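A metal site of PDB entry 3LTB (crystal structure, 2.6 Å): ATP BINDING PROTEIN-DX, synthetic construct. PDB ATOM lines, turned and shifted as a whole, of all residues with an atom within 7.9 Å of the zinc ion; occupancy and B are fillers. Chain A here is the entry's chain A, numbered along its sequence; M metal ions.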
ATOM      1  N   PRO A  24      36.734 -23.123 -30.020  1.00  0.00           N
ATOM      2  CA  PRO A  24      35.372 -22.711 -29.736  1.00  0.00           C
ATOM      3  C   PRO A  24      34.319 -23.713 -30.259  1.00  0.00           C
ATOM      4  O   PRO A  24      34.643 -24.664 -30.961  1.00  0.00           O
ATOM      5  CB  PRO A  24      35.256 -21.377 -30.468  1.00  0.00           C
ATOM      6  CG  PRO A  24      36.253 -21.466 -31.605  1.00  0.00           C
ATOM      7  CD  PRO A  24      37.319 -22.450 -31.198  1.00  0.00           C
ATOM      8  N   CYS A  25      33.067 -23.494 -29.885  1.00  0.00           N
ATOM      9  CA  CYS A  25      31.972 -24.286 -30.355  1.00  0.00           C
ATOM     10  C   CYS A  25      32.170 -24.774 -31.801  1.00  0.00           C
ATOM     11  O   CYS A  25      32.439 -23.966 -32.674  1.00  0.00           O
ATOM     12  CB  CYS A  25      30.702 -23.453 -30.274  1.00  0.00           C
ATOM     13  SG  CYS A  25      29.325 -24.313 -30.992  1.00  0.00           S
ATOM     14  N   VAL A  26      32.004 -26.064 -32.061  1.00  0.00           N
ATOM     15  CA  VAL A  26      32.179 -26.579 -33.418  1.00  0.00           C
ATOM     16  C   VAL A  26      31.150 -26.059 -34.446  1.00  0.00           C
ATOM     17  O   VAL A  26      31.419 -26.100 -35.647  1.00  0.00           O
ATOM     18  CB  VAL A  26      32.100 -28.138 -33.513  1.00  0.00           C
ATOM     19  CG1 VAL A  26      33.248 -28.817 -32.719  1.00  0.00           C
ATOM     20  CG2 VAL A  26      30.716 -28.619 -33.084  1.00  0.00           C
ATOM     21  N   LYS A  27      29.985 -25.587 -33.987  1.00  0.00           N
ATOM     22  CA  LYS A  27      28.903 -25.209 -34.901  1.00  0.00           C
ATOM     23  C   LYS A  27      28.980 -23.727 -35.252  1.00  0.00           C
ATOM     24  O   LYS A  27      29.014 -23.364 -36.432  1.00  0.00           O
ATOM     25  CB  LYS A  27      27.550 -25.545 -34.289  1.00  0.00           C
ATOM     26  CG  LYS A  27      26.346 -25.229 -35.154  1.00  0.00           C
ATOM     27  CD  LYS A  27      26.435 -25.910 -36.503  1.00  0.00           C
ATOM     28  CE  LYS A  27      25.213 -25.528 -37.330  1.00  0.00           C
ATOM     29  NZ  LYS A  27      25.279 -26.107 -38.707  1.00  0.00           N
ATOM     30  N   CYS A  28      29.007 -22.847 -34.243  1.00  0.00           N
ATOM     31  CA  CYS A  28      29.080 -21.414 -34.492  1.00  0.00           C
ATOM     32  C   CYS A  28      30.506 -20.856 -34.496  1.00  0.00           C
ATOM     33  O   CYS A  28      30.696 -19.711 -34.849  1.00  0.00           O
ATOM     34  CB  CYS A  28      28.234 -20.667 -33.449  1.00  0.00           C
ATOM     35  SG  CYS A  28      28.991 -20.621 -31.775  1.00  0.00           S
ATOM     36  N   LYS A  29      31.494 -21.634 -34.063  1.00  0.00           N
ATOM     37  CA  LYS A  29      32.896 -21.195 -34.106  1.00  0.00           C
ATOM     38  C   LYS A  29      33.244 -19.939 -33.328  1.00  0.00           C
ATOM     39  O   LYS A  29      34.331 -19.434 -33.469  1.00  0.00           O
ATOM     40  CB  LYS A  29      33.356 -20.886 -35.541  1.00  0.00           C
ATOM     41  CG  LYS A  29      32.702 -21.667 -36.645  1.00  0.00           C
ATOM     42  CD  LYS A  29      33.502 -22.895 -36.941  1.00  0.00           C
ATOM     43  CE  LYS A  29      32.989 -23.598 -38.163  1.00  0.00           C
ATOM     44  NZ  LYS A  29      33.449 -25.017 -38.025  1.00  0.00           N
ATOM     45  N   VAL A  30      32.346 -19.386 -32.544  1.00  0.00           N
ATOM     46  CA  VAL A  30      32.682 -18.199 -31.774  1.00  0.00           C
ATOM     47  C   VAL A  30      32.478 -18.446 -30.262  1.00  0.00           C
ATOM     48  O   VAL A  30      33.449 -18.314 -29.498  1.00  0.00           O
ATOM     49  CB  VAL A  30      31.872 -16.979 -32.243  1.00  0.00           C
ATOM     50  CG1 VAL A  30      32.085 -15.776 -31.289  1.00  0.00           C
ATOM     51  CG2 VAL A  30      32.279 -16.645 -33.674  1.00  0.00           C
ATOM     52  N   ALA A  31      31.262 -18.803 -29.838  1.00  0.00           N
ATOM     53  CA  ALA A  31      30.992 -19.082 -28.410  1.00  0.00           C
ATOM     54  C   ALA A  31      31.903 -20.197 -27.937  1.00  0.00           C
ATOM     55  O   ALA A  31      32.335 -21.053 -28.735  1.00  0.00           O
ATOM     56  CB  ALA A  31      29.508 -19.436 -28.153  1.00  0.00           C
ATOM     57  N   PRO A  32      32.264 -20.169 -26.649  1.00  0.00           N
ATOM     58  CA  PRO A  32      33.054 -21.282 -26.099  1.00  0.00           C
ATOM     59  C   PRO A  32      32.113 -22.449 -25.849  1.00  0.00           C
ATOM     60  O   PRO A  32      30.902 -22.284 -25.871  1.00  0.00           O
ATOM     61  CB  PRO A  32      33.611 -20.718 -24.781  1.00  0.00           C
ATOM     62  CG  PRO A  32      32.926 -19.398 -24.557  1.00  0.00           C
ATOM     63  CD  PRO A  32      32.336 -18.937 -25.845  1.00  0.00           C
ATOM     64  N   ARG A  33      32.663 -23.623 -25.611  1.00  0.00           N
ATOM     65  CA  ARG A  33      31.841 -24.814 -25.489  1.00  0.00           C
ATOM     66  C   ARG A  33      31.185 -24.981 -24.094  1.00  0.00           C
ATOM     67  O   ARG A  33      31.709 -24.525 -23.040  1.00  0.00           O
ATOM     68  CB  ARG A  33      32.690 -26.047 -25.797  1.00  0.00           C
ATOM     69  CG  ARG A  33      33.191 -26.118 -27.197  1.00  0.00           C
ATOM     70  CD  ARG A  33      34.245 -27.222 -27.395  1.00  0.00           C
ATOM     71  NE  ARG A  33      34.810 -27.093 -28.721  1.00  0.00           N
ATOM     72  CZ  ARG A  33      35.340 -28.089 -29.426  1.00  0.00           C
ATOM     73  NH1 ARG A  33      35.385 -29.334 -28.925  1.00  0.00           N
ATOM     74  NH2 ARG A  33      35.810 -27.827 -30.642  1.00  0.00           N
ATOM     75  N   ASP A  34      30.061 -25.687 -24.080  1.00  0.00           N
ATOM     76  CA  ASP A  34      29.485 -26.139 -22.846  1.00  0.00           C
ATOM     77  C   ASP A  34      30.420 -27.196 -22.254  1.00  0.00           C
ATOM     78  O   ASP A  34      31.256 -27.743 -22.956  1.00  0.00           O
ATOM     79  CB  ASP A  34      28.095 -26.745 -23.087  1.00  0.00           C
ATOM     80  CG  ASP A  34      27.310 -26.903 -21.789  1.00  0.00           C
ATOM     81  OD1 ASP A  34      27.722 -26.311 -20.780  1.00  0.00           O
ATOM     82  OD2 ASP A  34      26.297 -27.618 -21.768  1.00  0.00           O
ATOM     83  N   ASN A  46      31.100 -30.626 -27.580  1.00  0.00           N
ATOM     84  CA  ASN A  46      31.501 -30.004 -28.843  1.00  0.00           C
ATOM     85  C   ASN A  46      30.849 -28.642 -29.146  1.00  0.00           C
ATOM     86  O   ASN A  46      31.409 -27.825 -29.884  1.00  0.00           O
ATOM     87  CB  ASN A  46      31.228 -30.964 -30.014  1.00  0.00           C
ATOM     88  CG  ASN A  46      31.835 -32.285 -29.807  1.00  0.00           C
ATOM     89  OD1 ASN A  46      32.948 -32.407 -29.279  1.00  0.00           O
ATOM     90  ND2 ASN A  46      31.125 -33.332 -30.219  1.00  0.00           N
ATOM     91  N   MET A  47      29.647 -28.414 -28.605  1.00  0.00           N
ATOM     92  CA  MET A  47      28.929 -27.176 -28.884  1.00  0.00           C
ATOM     93  C   MET A  47      28.684 -26.298 -27.625  1.00  0.00           C
ATOM     94  O   MET A  47      28.634 -26.813 -26.496  1.00  0.00           O
ATOM     95  CB  MET A  47      27.595 -27.526 -29.549  1.00  0.00           C
ATOM     96  CG  MET A  47      27.704 -27.837 -31.037  1.00  0.00           C
ATOM     97  SD  MET A  47      26.081 -28.167 -31.816  1.00  0.00           S
ATOM     98  CE  MET A  47      25.600 -29.691 -30.960  1.00  0.00           C
ATOM     99  N   CYS A  48      28.518 -24.983 -27.833  1.00  0.00           N
ATOM    100  CA  CYS A  48      28.014 -24.111 -26.754  1.00  0.00           C
ATOM    101  C   CYS A  48      26.574 -24.531 -26.488  1.00  0.00           C
ATOM    102  O   CYS A  48      26.022 -25.326 -27.240  1.00  0.00           O
ATOM    103  CB  CYS A  48      28.082 -22.613 -27.121  1.00  0.00           C
ATOM    104  SG  CYS A  48      27.073 -22.151 -28.555  1.00  0.00           S
ATOM    105  N   LYS A  49      25.945 -24.025 -25.428  1.00  0.00           N
ATOM    106  CA  LYS A  49      24.580 -24.437 -25.119  1.00  0.00           C
ATOM    107  C   LYS A  49      23.579 -23.951 -26.170  1.00  0.00           C
ATOM    108  O   LYS A  49      22.627 -24.662 -26.497  1.00  0.00           O
ATOM    109  CB  LYS A  49      24.147 -23.935 -23.740  1.00  0.00           C
ATOM    110  CG  LYS A  49      22.947 -24.694 -23.157  1.00  0.00           C
ATOM    111  CD  LYS A  49      23.374 -25.934 -22.380  1.00  0.00           C
ATOM    112  CE  LYS A  49      22.250 -26.929 -22.355  1.00  0.00           C
ATOM    113  NZ  LYS A  49      22.632 -28.293 -21.816  1.00  0.00           N
ATOM    114  N   THR A  50      23.761 -22.738 -26.691  1.00  0.00           N
ATOM    115  CA  THR A  50      22.783 -22.194 -27.609  1.00  0.00           C
ATOM    116  C   THR A  50      22.740 -23.104 -28.845  1.00  0.00           C
ATOM    117  O   THR A  50      21.663 -23.440 -29.345  1.00  0.00           O
ATOM    118  CB  THR A  50      23.175 -20.771 -28.078  1.00  0.00           C
ATOM    119  OG1 THR A  50      23.337 -19.905 -26.948  1.00  0.00           O
ATOM    120  CG2 THR A  50      22.106 -20.193 -29.014  1.00  0.00           C
ATOM    121  N   CYS A  51      23.898 -23.503 -29.349  1.00  0.00           N
ATOM    122  CA  CYS A  51      23.914 -24.300 -30.574  1.00  0.00           C
ATOM    123  C   CYS A  51      23.434 -25.702 -30.318  1.00  0.00           C
ATOM    124  O   CYS A  51      22.804 -26.302 -31.203  1.00  0.00           O
ATOM    125  CB  CYS A  51      25.307 -24.332 -31.233  1.00  0.00           C
ATOM    126  SG  CYS A  51      25.805 -22.754 -31.963  1.00  0.00           S
ATOM    127  N   PHE A  52      23.747 -26.242 -29.126  1.00  0.00           N
ATOM    128  CA  PHE A  52      23.225 -27.545 -28.735  1.00  0.00           C
ATOM    129  C   PHE A  52      21.687 -27.582 -28.724  1.00  0.00           C
ATOM    130  O   PHE A  52      21.083 -28.417 -29.428  1.00  0.00           O
ATOM    131  CB  PHE A  52      23.771 -28.017 -27.405  1.00  0.00           C
ATOM    132  CG  PHE A  52      23.188 -29.331 -26.975  1.00  0.00           C
ATOM    133  CD1 PHE A  52      23.436 -30.498 -27.725  1.00  0.00           C
ATOM    134  CD2 PHE A  52      22.368 -29.413 -25.822  1.00  0.00           C
ATOM    135  CE1 PHE A  52      22.889 -31.755 -27.332  1.00  0.00           C
ATOM    136  CE2 PHE A  52      21.804 -30.633 -25.426  1.00  0.00           C
ATOM    137  CZ  PHE A  52      22.064 -31.829 -26.180  1.00  0.00           C
HETATM  138 ZN    ZN M   1      27.858 -22.476 -30.855  1.00  0.00          ZN
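Within 4 Å of the zinc ion: Cys 25, Cys 28, Cys 48 and Cys 51.
The zinc ion is bound by the side-chain sulfur (SG) of Cys 51, the side-chain sulfur (SG) of Cys 25, the side-chain sulfur (SG) of Cys 28 and the side-chain sulfur (SG) of Cys 48.
The zinc ion has four donor atoms within binding distance.
The side-chain sulfur of Cys 28 lies close to the backbone NH of Val 30.
The backbone NH (N) of Ala 31 sits close to the side-chain sulfur (SG) of Cys 28, 3.5 Å away.
The backbone NH (N) of Lys 27 sits close to the side-chain sulfur (SG) of Cys 25.
N of Cys 25 sits at hydrogen-bond distance from O of Ala 31, at 2.8 Å.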
